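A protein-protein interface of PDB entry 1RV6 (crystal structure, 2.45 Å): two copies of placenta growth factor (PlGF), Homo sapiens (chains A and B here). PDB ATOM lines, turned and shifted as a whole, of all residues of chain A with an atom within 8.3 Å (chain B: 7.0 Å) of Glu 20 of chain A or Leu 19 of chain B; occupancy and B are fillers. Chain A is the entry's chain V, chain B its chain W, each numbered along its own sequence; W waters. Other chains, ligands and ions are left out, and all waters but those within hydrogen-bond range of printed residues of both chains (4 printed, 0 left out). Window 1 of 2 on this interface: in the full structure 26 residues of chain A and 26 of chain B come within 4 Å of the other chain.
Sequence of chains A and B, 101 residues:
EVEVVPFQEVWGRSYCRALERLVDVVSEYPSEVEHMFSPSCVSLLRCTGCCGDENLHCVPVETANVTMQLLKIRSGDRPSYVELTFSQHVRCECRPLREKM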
ATOM      1  N   ARG A  17      -5.110 -27.479  -1.874  1.00  0.00           N
ATOM      2  CA  ARG A  17      -4.396 -26.936  -3.026  1.00  0.00           C
ATOM      3  C   ARG A  17      -2.899 -27.047  -2.953  1.00  0.00           C
ATOM      4  O   ARG A  17      -2.337 -27.222  -1.863  1.00  0.00           O
ATOM      5  CB  ARG A  17      -4.763 -25.480  -3.243  1.00  0.00           C
ATOM      6  CG  ARG A  17      -4.669 -24.614  -2.031  1.00  0.00           C
ATOM      7  CD  ARG A  17      -4.235 -23.244  -2.459  1.00  0.00           C
ATOM      8  NE  ARG A  17      -4.469 -22.191  -1.498  1.00  0.00           N
ATOM      9  CZ  ARG A  17      -4.037 -20.948  -1.643  1.00  0.00           C
ATOM     10  NH1 ARG A  17      -3.325 -20.599  -2.721  1.00  0.00           N
ATOM     11  NH2 ARG A  17      -4.314 -20.046  -0.697  1.00  0.00           N
ATOM     12  N   ALA A  18      -2.260 -26.943  -4.120  1.00  0.00           N
ATOM     13  CA  ALA A  18      -0.801 -26.904  -4.195  1.00  0.00           C
ATOM     14  C   ALA A  18      -0.345 -25.490  -3.894  1.00  0.00           C
ATOM     15  O   ALA A  18      -0.495 -24.597  -4.729  1.00  0.00           O
ATOM     16  CB  ALA A  18      -0.310 -27.342  -5.558  1.00  0.00           C
ATOM     17  N   LEU A  19       0.237 -25.323  -2.710  1.00  0.00           N
ATOM     18  CA  LEU A  19       0.676 -24.039  -2.154  1.00  0.00           C
ATOM     19  C   LEU A  19       2.194 -23.939  -2.037  1.00  0.00           C
ATOM     20  O   LEU A  19       2.824 -24.875  -1.540  1.00  0.00           O
ATOM     21  CB  LEU A  19       0.119 -23.943  -0.733  1.00  0.00           C
ATOM     22  CG  LEU A  19      -0.013 -22.581  -0.087  1.00  0.00           C
ATOM     23  CD1 LEU A  19      -0.963 -21.733  -0.895  1.00  0.00           C
ATOM     24  CD2 LEU A  19      -0.516 -22.722   1.322  1.00  0.00           C
ATOM     25  N   GLU A  20       2.778 -22.816  -2.457  1.00  0.00           N
ATOM     26  CA  GLU A  20       4.203 -22.541  -2.213  1.00  0.00           C
ATOM     27  C   GLU A  20       4.505 -22.668  -0.734  1.00  0.00           C
ATOM     28  O   GLU A  20       3.877 -21.974   0.070  1.00  0.00           O
ATOM     29  CB  GLU A  20       4.553 -21.113  -2.597  1.00  0.00           C
ATOM     30  CG  GLU A  20       5.166 -20.938  -3.966  1.00  0.00           C
ATOM     31  CD  GLU A  20       5.768 -19.565  -4.132  1.00  0.00           C
ATOM     32  OE1 GLU A  20       4.997 -18.595  -4.296  1.00  0.00           O
ATOM     33  OE2 GLU A  20       7.005 -19.459  -4.121  1.00  0.00           O
ATOM     34  N   ARG A  21       5.415 -23.561  -0.351  1.00  0.00           N
ATOM     35  CA  ARG A  21       6.064 -23.382   0.935  1.00  0.00           C
ATOM     36  C   ARG A  21       7.583 -23.515   0.794  1.00  0.00           C
ATOM     37  O   ARG A  21       8.078 -24.024  -0.218  1.00  0.00           O
ATOM     38  CB  ARG A  21       5.455 -24.253   2.049  1.00  0.00           C
ATOM     39  CG  ARG A  21       5.699 -25.756   1.989  1.00  0.00           C
ATOM     40  CD  ARG A  21       5.337 -26.436   3.322  1.00  0.00           C
ATOM     41  NE  ARG A  21       5.260 -27.900   3.278  1.00  0.00           N
ATOM     42  CZ  ARG A  21       4.119 -28.627   3.274  1.00  0.00           C
ATOM     43  NH1 ARG A  21       2.916 -28.040   3.304  1.00  0.00           N
ATOM     44  NH2 ARG A  21       4.186 -29.962   3.240  1.00  0.00           N
ATOM     45  N   LEU A  22       8.306 -23.038   1.804  1.00  0.00           N
ATOM     46  CA  LEU A  22       9.752 -23.120   1.814  1.00  0.00           C
ATOM     47  C   LEU A  22      10.156 -24.444   2.408  1.00  0.00           C
ATOM     48  O   LEU A  22       9.728 -24.794   3.495  1.00  0.00           O
ATOM     49  CB  LEU A  22      10.389 -21.966   2.583  1.00  0.00           C
ATOM     50  CG  LEU A  22      10.148 -20.594   1.935  1.00  0.00           C
ATOM     51  CD1 LEU A  22      11.146 -19.553   2.465  1.00  0.00           C
ATOM     52  CD2 LEU A  22      10.219 -20.697   0.429  1.00  0.00           C
ATOM     53  N   VAL A  23      10.980 -25.185   1.662  1.00  0.00           N
ATOM     54  CA  VAL A  23      11.432 -26.512   2.066  1.00  0.00           C
ATOM     55  C   VAL A  23      12.951 -26.521   2.143  1.00  0.00           C
ATOM     56  O   VAL A  23      13.625 -26.061   1.221  1.00  0.00           O
ATOM     57  CB  VAL A  23      10.973 -27.589   1.030  1.00  0.00           C
ATOM     58  CG1 VAL A  23      11.487 -28.962   1.409  1.00  0.00           C
ATOM     59  CG2 VAL A  23       9.436 -27.614   0.882  1.00  0.00           C
ATOM     60  N   VAL A  42      14.379 -23.978  -0.481  1.00  0.00           N
ATOM     61  CA  VAL A  42      13.853 -23.611  -1.773  1.00  0.00           C
ATOM     62  C   VAL A  42      12.344 -23.570  -1.700  1.00  0.00           C
ATOM     63  O   VAL A  42      11.738 -24.211  -0.828  1.00  0.00           O
ATOM     64  CB  VAL A  42      14.291 -24.613  -2.872  1.00  0.00           C
ATOM     65  CG1 VAL A  42      15.795 -24.465  -3.146  1.00  0.00           C
ATOM     66  CG2 VAL A  42      13.937 -26.062  -2.493  1.00  0.00           C
ATOM     67  N   SER A  43      11.743 -22.819  -2.622  1.00  0.00           N
ATOM     68  CA  SER A  43      10.287 -22.778  -2.760  1.00  0.00           C
ATOM     69  C   SER A  43       9.727 -23.941  -3.576  1.00  0.00           C
ATOM     70  O   SER A  43      10.043 -24.078  -4.765  1.00  0.00           O
ATOM     71  CB  SER A  43       9.865 -21.492  -3.442  1.00  0.00           C
ATOM     72  OG  SER A  43       8.465 -21.434  -3.450  1.00  0.00           O
ATOM     73  N   LEU A  44       8.872 -24.746  -2.952  1.00  0.00           N
ATOM     74  CA  LEU A  44       8.186 -25.846  -3.640  1.00  0.00           C
ATOM     75  C   LEU A  44       6.660 -25.766  -3.495  1.00  0.00           C
ATOM     76  O   LEU A  44       6.161 -25.316  -2.473  1.00  0.00           O
ATOM     77  CB  LEU A  44       8.691 -27.222  -3.129  1.00  0.00           C
ATOM     78  CG  LEU A  44      10.164 -27.586  -3.408  1.00  0.00           C
ATOM     79  CD1 LEU A  44      10.502 -28.943  -2.882  1.00  0.00           C
ATOM     80  CD2 LEU A  44      10.482 -27.519  -4.882  1.00  0.00           C
ATOM     81  N   LEU A  45       5.927 -26.209  -4.517  1.00  0.00           N
ATOM     82  CA  LEU A  45       4.464 -26.323  -4.425  1.00  0.00           C
ATOM     83  C   LEU A  45       4.068 -27.585  -3.641  1.00  0.00           C
ATOM     84  O   LEU A  45       4.490 -28.714  -3.977  1.00  0.00           O
ATOM     85  CB  LEU A  45       3.850 -26.308  -5.817  1.00  0.00           C
ATOM     86  CG  LEU A  45       4.056 -24.951  -6.516  1.00  0.00           C
ATOM     87  CD1 LEU A  45       3.953 -25.057  -8.028  1.00  0.00           C
ATOM     88  CD2 LEU A  45       3.079 -23.924  -6.011  1.00  0.00           C
ATOM     89  N   ARG A  46       3.309 -27.412  -2.564  1.00  0.00           N
ATOM     90  CA  ARG A  46       2.919 -28.572  -1.748  1.00  0.00           C
ATOM     91  C   ARG A  46       1.435 -28.549  -1.439  1.00  0.00           C
ATOM     92  O   ARG A  46       0.845 -27.479  -1.196  1.00  0.00           O
ATOM     93  CB  ARG A  46       3.737 -28.648  -0.437  1.00  0.00           C
ATOM     94  CG  ARG A  46       5.223 -29.047  -0.615  1.00  0.00           C
ATOM     95  CD  ARG A  46       5.361 -30.548  -0.815  1.00  0.00           C
ATOM     96  NE  ARG A  46       6.705 -31.070  -1.077  1.00  0.00           N
ATOM     97  CZ  ARG A  46       7.270 -31.157  -2.285  1.00  0.00           C
ATOM     98  NH1 ARG A  46       6.641 -30.665  -3.357  1.00  0.00           N
ATOM     99  NH2 ARG A  46       8.474 -31.725  -2.419  1.00  0.00           N
ATOM    100  N   CYS A  47       0.842 -29.733  -1.472  1.00  0.00           N
ATOM    101  CA  CYS A  47      -0.565 -29.915  -1.183  1.00  0.00           C
ATOM    102  C   CYS A  47      -0.878 -29.636   0.296  1.00  0.00           C
ATOM    103  O   CYS A  47      -0.318 -30.277   1.195  1.00  0.00           O
ATOM    104  CB  CYS A  47      -0.956 -31.343  -1.565  1.00  0.00           C
ATOM    105  SG  CYS A  47      -1.058 -31.618  -3.354  1.00  0.00           S
ATOM    106  N   THR A  48      -1.788 -28.699   0.547  1.00  0.00           N
ATOM    107  CA  THR A  48      -2.204 -28.375   1.922  1.00  0.00           C
ATOM    108  C   THR A  48      -3.695 -27.998   1.945  1.00  0.00           C
ATOM    109  O   THR A  48      -4.210 -27.493   0.944  1.00  0.00           O
ATOM    110  CB  THR A  48      -1.298 -27.229   2.454  1.00  0.00           C
ATOM    111  OG1 THR A  48      -1.753 -26.745   3.727  1.00  0.00           O
ATOM    112  CG2 THR A  48      -1.449 -26.042   1.607  1.00  0.00           C
ATOM    113  N   GLN A  88       7.409 -31.203  -7.675  1.00  0.00           N
ATOM    114  CA  GLN A  88       6.322 -30.229  -7.428  1.00  0.00           C
ATOM    115  C   GLN A  88       4.964 -30.911  -7.358  1.00  0.00           C
ATOM    116  O   GLN A  88       4.690 -31.798  -8.148  1.00  0.00           O
ATOM    117  CB  GLN A  88       6.199 -29.199  -8.569  1.00  0.00           C
ATOM    118  CG  GLN A  88       7.330 -28.224  -8.801  1.00  0.00           C
ATOM    119  CD  GLN A  88       7.365 -27.078  -7.832  1.00  0.00           C
ATOM    120  OE1 GLN A  88       6.953 -27.219  -6.680  1.00  0.00           O
ATOM    121  NE2 GLN A  88       7.877 -25.934  -8.281  1.00  0.00           N
ATOM    122  N   HIS A  89       4.079 -30.456  -6.472  1.00  0.00           N
ATOM    123  CA  HIS A  89       2.697 -30.917  -6.515  1.00  0.00           C
ATOM    124  C   HIS A  89       1.892 -30.093  -7.525  1.00  0.00           C
ATOM    125  O   HIS A  89       1.785 -28.875  -7.391  1.00  0.00           O
ATOM    126  CB  HIS A  89       2.040 -30.898  -5.126  1.00  0.00           C
ATOM    127  CG  HIS A  89       2.687 -31.803  -4.110  1.00  0.00           C
ATOM    128  ND1 HIS A  89       2.362 -31.762  -2.770  1.00  0.00           N
ATOM    129  CD2 HIS A  89       3.649 -32.751  -4.228  1.00  0.00           C
ATOM    130  CE1 HIS A  89       3.074 -32.665  -2.112  1.00  0.00           C
ATOM    131  NE2 HIS A  89       3.869 -33.271  -2.972  1.00  0.00           N
ATOM    132  N   ARG B  13      13.119 -16.296  -4.195  1.00  0.00           N
ATOM    133  CA  ARG B  13      11.863 -16.912  -3.822  1.00  0.00           C
ATOM    134  C   ARG B  13      11.865 -17.530  -2.444  1.00  0.00           C
ATOM    135  O   ARG B  13      10.798 -17.806  -1.888  1.00  0.00           O
ATOM    136  CB  ARG B  13      11.488 -17.970  -4.828  1.00  0.00           C
ATOM    137  CG  ARG B  13      10.651 -17.415  -5.921  1.00  0.00           C
ATOM    138  CD  ARG B  13      10.654 -18.302  -7.104  1.00  0.00           C
ATOM    139  NE  ARG B  13       9.317 -18.431  -7.640  1.00  0.00           N
ATOM    140  CZ  ARG B  13       9.061 -18.780  -8.879  1.00  0.00           C
ATOM    141  NH1 ARG B  13      10.076 -19.029  -9.726  1.00  0.00           N
ATOM    142  NH2 ARG B  13       7.792 -18.877  -9.268  1.00  0.00           N
ATOM    143  N   SER B  14      13.049 -17.757  -1.886  1.00  0.00           N
ATOM    144  CA  SER B  14      13.102 -18.363  -0.572  1.00  0.00           C
ATOM    145  C   SER B  14      13.812 -17.522   0.506  1.00  0.00           C
ATOM    146  O   SER B  14      14.051 -18.025   1.611  1.00  0.00           O
ATOM    147  CB  SER B  14      13.782 -19.707  -0.698  1.00  0.00           C
ATOM    148  OG  SER B  14      15.152 -19.483  -0.969  1.00  0.00           O
ATOM    149  N   ARG B  17      10.131 -13.503   2.881  1.00  0.00           N
ATOM    150  CA  ARG B  17       8.927 -13.220   2.097  1.00  0.00           C
ATOM    151  C   ARG B  17       7.663 -13.516   2.904  1.00  0.00           C
ATOM    152  O   ARG B  17       7.639 -14.431   3.706  1.00  0.00           O
ATOM    153  CB  ARG B  17       8.860 -14.223   0.951  1.00  0.00           C
ATOM    154  CG  ARG B  17       9.538 -13.852  -0.279  1.00  0.00           C
ATOM    155  CD  ARG B  17       8.779 -14.317  -1.496  1.00  0.00           C
ATOM    156  NE  ARG B  17       8.882 -15.745  -1.740  1.00  0.00           N
ATOM    157  CZ  ARG B  17       8.076 -16.421  -2.574  1.00  0.00           C
ATOM    158  NH1 ARG B  17       7.076 -15.806  -3.202  1.00  0.00           N
ATOM    159  NH2 ARG B  17       8.254 -17.719  -2.773  1.00  0.00           N
ATOM    160  N   ALA B  18       6.594 -12.784   2.637  1.00  0.00           N
ATOM    161  CA  ALA B  18       5.286 -13.114   3.189  1.00  0.00           C
ATOM    162  C   ALA B  18       4.598 -14.129   2.282  1.00  0.00           C
ATOM    163  O   ALA B  18       4.302 -13.819   1.134  1.00  0.00           O
ATOM    164  CB  ALA B  18       4.439 -11.848   3.309  1.00  0.00           C
ATOM    165  N   LEU B  19       4.359 -15.341   2.781  1.00  0.00           N
ATOM    166  CA  LEU B  19       3.636 -16.355   1.998  1.00  0.00           C
ATOM    167  C   LEU B  19       2.353 -16.813   2.681  1.00  0.00           C
ATOM    168  O   LEU B  19       2.241 -16.816   3.923  1.00  0.00           O
ATOM    169  CB  LEU B  19       4.502 -17.588   1.692  1.00  0.00           C
ATOM    170  CG  LEU B  19       5.643 -17.531   0.664  1.00  0.00           C
ATOM    171  CD1 LEU B  19       6.181 -18.912   0.455  1.00  0.00           C
ATOM    172  CD2 LEU B  19       5.157 -17.006  -0.648  1.00  0.00           C
ATOM    173  N   GLU B  20       1.380 -17.191   1.855  1.00  0.00           N
ATOM    174  CA  GLU B  20       0.153 -17.809   2.335  1.00  0.00           C
ATOM    175  C   GLU B  20       0.477 -19.116   3.031  1.00  0.00           C
ATOM    176  O   GLU B  20       1.196 -19.969   2.465  1.00  0.00           O
ATOM    177  CB  GLU B  20      -0.783 -18.129   1.156  1.00  0.00           C
ATOM    178  CG  GLU B  20      -1.483 -16.955   0.492  1.00  0.00           C
ATOM    179  CD  GLU B  20      -2.521 -17.428  -0.515  1.00  0.00           C
ATOM    180  OE1 GLU B  20      -2.142 -17.849  -1.647  1.00  0.00           O
ATOM    181  OE2 GLU B  20      -3.723 -17.423  -0.165  1.00  0.00           O
ATOM    182  N   ARG B  21      -0.052 -19.276   4.244  1.00  0.00           N
ATOM    183  CA  ARG B  21      -0.137 -20.580   4.895  1.00  0.00           C
ATOM    184  C   ARG B  21      -1.465 -20.742   5.660  1.00  0.00           C
ATOM    185  O   ARG B  21      -2.076 -19.748   6.048  1.00  0.00           O
ATOM    186  CB  ARG B  21       1.100 -20.860   5.764  1.00  0.00           C
ATOM    187  CG  ARG B  21       1.220 -20.084   7.021  1.00  0.00           C
ATOM    188  CD  ARG B  21       2.163 -20.748   8.006  1.00  0.00           C
ATOM    189  NE  ARG B  21       1.993 -20.151   9.327  1.00  0.00           N
ATOM    190  CZ  ARG B  21       2.936 -19.490   9.990  1.00  0.00           C
ATOM    191  NH1 ARG B  21       4.170 -19.358   9.490  1.00  0.00           N
ATOM    192  NH2 ARG B  21       2.639 -18.974  11.179  1.00  0.00           N
ATOM    193  N   LEU B  22      -1.915 -21.980   5.855  1.00  0.00           N
ATOM    194  CA  LEU B  22      -3.231 -22.200   6.457  1.00  0.00           C
ATOM    195  C   LEU B  22      -3.120 -22.132   7.971  1.00  0.00           C
ATOM    196  O   LEU B  22      -2.274 -22.797   8.574  1.00  0.00           O
ATOM    197  CB  LEU B  22      -3.873 -23.527   6.001  1.00  0.00           C
ATOM    198  CG  LEU B  22      -3.902 -23.679   4.478  1.00  0.00           C
ATOM    199  CD1 LEU B  22      -4.658 -24.893   3.996  1.00  0.00           C
ATOM    200  CD2 LEU B  22      -4.423 -22.408   3.815  1.00  0.00           C
ATOM    201  N   SER B  43      -6.484 -18.954   4.963  1.00  0.00           N
ATOM    202  CA  SER B  43      -5.180 -18.593   4.424  1.00  0.00           C
ATOM    203  C   SER B  43      -4.722 -17.198   4.853  1.00  0.00           C
ATOM    204  O   SER B  43      -5.371 -16.206   4.507  1.00  0.00           O
ATOM    205  CB  SER B  43      -5.243 -18.648   2.909  1.00  0.00           C
ATOM    206  OG  SER B  43      -4.025 -18.202   2.358  1.00  0.00           O
ATOM    207  N   LEU B  44      -3.617 -17.105   5.586  1.00  0.00           N
ATOM    208  CA  LEU B  44      -3.036 -15.775   5.929  1.00  0.00           C
ATOM    209  C   LEU B  44      -1.591 -15.586   5.431  1.00  0.00           C
ATOM    210  O   LEU B  44      -0.842 -16.558   5.342  1.00  0.00           O
ATOM    211  CB  LEU B  44      -3.057 -15.529   7.440  1.00  0.00           C
ATOM    212  CG  LEU B  44      -4.411 -15.664   8.130  1.00  0.00           C
ATOM    213  CD1 LEU B  44      -4.226 -15.679   9.639  1.00  0.00           C
ATOM    214  CD2 LEU B  44      -5.323 -14.526   7.711  1.00  0.00           C
ATOM    215  N   LEU B  45      -1.195 -14.348   5.136  1.00  0.00           N
ATOM    216  CA  LEU B  45       0.211 -14.051   4.844  1.00  0.00           C
ATOM    217  C   LEU B  45       1.061 -14.141   6.104  1.00  0.00           C
ATOM    218  O   LEU B  45       0.774 -13.463   7.091  1.00  0.00           O
ATOM    219  CB  LEU B  45       0.354 -12.670   4.194  1.00  0.00           C
ATOM    220  CG  LEU B  45      -0.325 -12.501   2.817  1.00  0.00           C
ATOM    221  CD1 LEU B  45      -0.188 -11.046   2.304  1.00  0.00           C
ATOM    222  CD2 LEU B  45       0.256 -13.481   1.777  1.00  0.00           C
ATOM    223  N   ARG B  46       2.085 -14.997   6.065  1.00  0.00           N
ATOM    224  CA  ARG B  46       3.096 -15.131   7.142  1.00  0.00           C
ATOM    225  C   ARG B  46       4.541 -15.084   6.629  1.00  0.00           C
ATOM    226  O   ARG B  46       4.881 -15.723   5.608  1.00  0.00           O
ATOM    227  CB  ARG B  46       2.921 -16.449   7.909  1.00  0.00           C
ATOM    228  CG  ARG B  46       1.595 -16.523   8.663  1.00  0.00           C
ATOM    229  CD  ARG B  46       1.634 -15.836   9.990  1.00  0.00           C
ATOM    230  NE  ARG B  46       0.601 -14.828  10.074  1.00  0.00           N
ATOM    231  CZ  ARG B  46      -0.471 -14.945  10.821  1.00  0.00           C
ATOM    232  NH1 ARG B  46      -0.646 -16.041  11.561  1.00  0.00           N
ATOM    233  NH2 ARG B  46      -1.364 -13.966  10.841  1.00  0.00           N
ATOM    234  N   CYS B  47       5.386 -14.348   7.349  1.00  0.00           N
ATOM    235  CA  CYS B  47       6.788 -14.190   6.973  1.00  0.00           C
ATOM    236  C   CYS B  47       7.469 -15.523   7.047  1.00  0.00           C
ATOM    237  O   CYS B  47       7.341 -16.255   8.059  1.00  0.00           O
ATOM    238  CB  CYS B  47       7.496 -13.208   7.898  1.00  0.00           C
ATOM    239  SG  CYS B  47       6.993 -11.536   7.575  1.00  0.00           S
ATOM    240  N   THR B  48       8.211 -15.832   5.990  1.00  0.00           N
ATOM    241  CA  THR B  48       8.925 -17.105   5.934  1.00  0.00           C
ATOM    242  C   THR B  48      10.168 -16.961   5.076  1.00  0.00           C
ATOM    243  O   THR B  48      10.194 -16.110   4.178  1.00  0.00           O
ATOM    244  CB  THR B  48       7.967 -18.181   5.413  1.00  0.00           C
ATOM    245  OG1 THR B  48       8.584 -19.467   5.499  1.00  0.00           O
ATOM    246  CG2 THR B  48       7.628 -17.960   3.900  1.00  0.00           C
ATOM    247  N   HIS B  89       0.875 -10.658   7.720  1.00  0.00           N
ATOM    248  CA  HIS B  89       2.210 -10.083   7.545  1.00  0.00           C
ATOM    249  C   HIS B  89       2.308  -9.488   6.146  1.00  0.00           C
ATOM    250  O   HIS B  89       2.077 -10.177   5.165  1.00  0.00           O
ATOM    251  CB  HIS B  89       3.304 -11.130   7.758  1.00  0.00           C
ATOM    252  CG  HIS B  89       3.267 -11.787   9.105  1.00  0.00           C
ATOM    253  ND1 HIS B  89       4.144 -12.794   9.463  1.00  0.00           N
ATOM    254  CD2 HIS B  89       2.467 -11.581  10.181  1.00  0.00           C
ATOM    255  CE1 HIS B  89       3.888 -13.176  10.703  1.00  0.00           C
ATOM    256  NE2 HIS B  89       2.879 -12.451  11.163  1.00  0.00           N
ATOM    257  N   CYS B  92       8.431  -8.034   5.431  1.00  0.00           N
ATOM    258  CA  CYS B  92       9.230  -8.946   6.217  1.00  0.00           C
ATOM    259  C   CYS B  92      10.667  -8.543   6.058  1.00  0.00           C
ATOM    260  O   CYS B  92      11.085  -8.047   5.002  1.00  0.00           O
ATOM    261  CB  CYS B  92       9.083 -10.372   5.672  1.00  0.00           C
ATOM    262  SG  CYS B  92       7.417 -11.037   5.640  1.00  0.00           S
HETATM  263  O   HOH W   1       2.041 -20.104  -0.379  1.00  0.00           O
HETATM  264  O   HOH W   2       7.496 -21.884   4.182  1.00  0.00           O
HETATM  265  O   HOH W   3       2.933 -21.877   2.509  1.00  0.00           O
HETATM  266  O   HOH W   4      -0.337 -24.194   5.102  1.00  0.00           O
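Printed residues of chain B within 4 Å of Arg 17 of chain A: Glu 20 (2.7 Å) and Ser 43 (3.6 Å).
Of the printed residues of chain A, Ser 14 of chain B touches Leu 22 (3.4 Å).
No residue of chain A comes within 4 Å of Ala 18 of chain B.
Leu 19 of chain B touches just one residue of chain A: Glu 20 (3.9 Å).
The nearest residue of chain A that does not touch Leu 19 of chain B is Leu 22 of chain A (4.4 Å).
Arg 17 of chain A touches Glu 20 of chain B, and with the chains exchanged Glu 20 of chain A touches Arg 17 of chain B.
Arg 17 of chain A touches Ser 43 of chain B, and with the chains exchanged Ser 43 of chain A touches Arg 17 of chain B.
Leu 19 of chain A touches Glu 20 of chain B, and with the chains exchanged Glu 20 of chain A touches Leu 19 of chain B.
Leu 22 of chain A touches Thr 48 of chain B, and with the chains exchanged Thr 48 of chain A touches Leu 22 of chain B.
Positions printed for both chains: 17, 18, 19, 20, 21, 22, 43, 44, 45, 46, 47, 48 and 89.
Of the 10 pairs that touch across the chains among the printed residues, 8 have their exchanged pair printed and touching as well.
The backbone NH (N) of Leu 19 of chain A sits at hydrogen-bond distance from the backbone carbonyl oxygen (O) of Arg 46 of chain A (2.7 Å).
NH2 of Arg 17 of chain B lies within hydrogen-bond range of O of Arg 13 of chain B.
The backbone NH of Thr 48 of chain A lies within hydrogen-bond range of the backbone carbonyl oxygen of Arg 17 of chain A (2.9 Å).
OG of Ser 43 of chain B is in hydrogen-bond range of OE2 of Glu 20 of chain B, at 2.7 Å.
The side-chain carboxylate (OE2) of Glu 20 of chain A sits at hydrogen-bond distance from the side-chain hydroxyl (OG) of Ser 43 of chain A.
The backbone carbonyl oxygen (O) of Leu 19 of chain B sits at hydrogen-bond distance from the backbone NH (N) of Arg 46 of chain B, 2.8 Å away.
Of the 16 printed residues of chain A, 6 touch a printed residue of chain B.
Printed residues of chain A that touch a printed residue of chain B: Arg 17, Leu 19, Glu 20, Leu 22, Ser 43 and Thr 48.
Hydrophobic or aromatic side chains of chain A that line the printed part of chain B: Leu 19 and Leu 22.
Printed residues of chain B that touch a printed residue of chain A: Arg 13, Ser 14, Arg 17, Leu 19, Glu 20, Leu 22, Ser 43 and Thr 48.
Among the printed residues, merely in contact across the chains: Arg 17 of chain A with Ser 43 of chain B (3.6 Å), Leu 19 of chain A with Glu 20 of chain B (3.4 Å), Glu 20 of chain A with Leu 19 of chain B (3.9 Å), Leu 22 of chain A with Arg 13 of chain B (3.7 Å), Leu 22 of chain A with Ser 14 of chain B (3.4 Å), Leu 22 of chain A with Thr 48 of chain B (3.8 Å), Ser 43 of chain A with Arg 17 of chain B (3.8 Å) and Thr 48 of chain A with Leu 22 of chain B (3.5 Å).
NH2 of Arg 17 of chain A lies within salt-bridge range of OE2 of Glu 20 of chain B.
The guanidinium group of Arg 17 of chain B lies within salt-bridge range of the side-chain carboxylate of Glu 20 of chain A (2.5 Å).
Water W3 lies within hydrogen-bond range of O of Glu 20 of chain B and O of Glu 20 of chain A.
Water W1 bridges O of Glu 20 of chain A (2.7 Å) and O of Glu 20 of chain B (3.0 Å).
Water W2 bridges the backbone NH of Leu 22 of chain A (2.8 Å) and the side-chain hydroxyl of Thr 48 of chain B (3.0 Å).
Water W4 bridges N of Leu 22 of chain B (2.8 Å) and OG1 of Thr 48 of chain A (3.2 Å).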
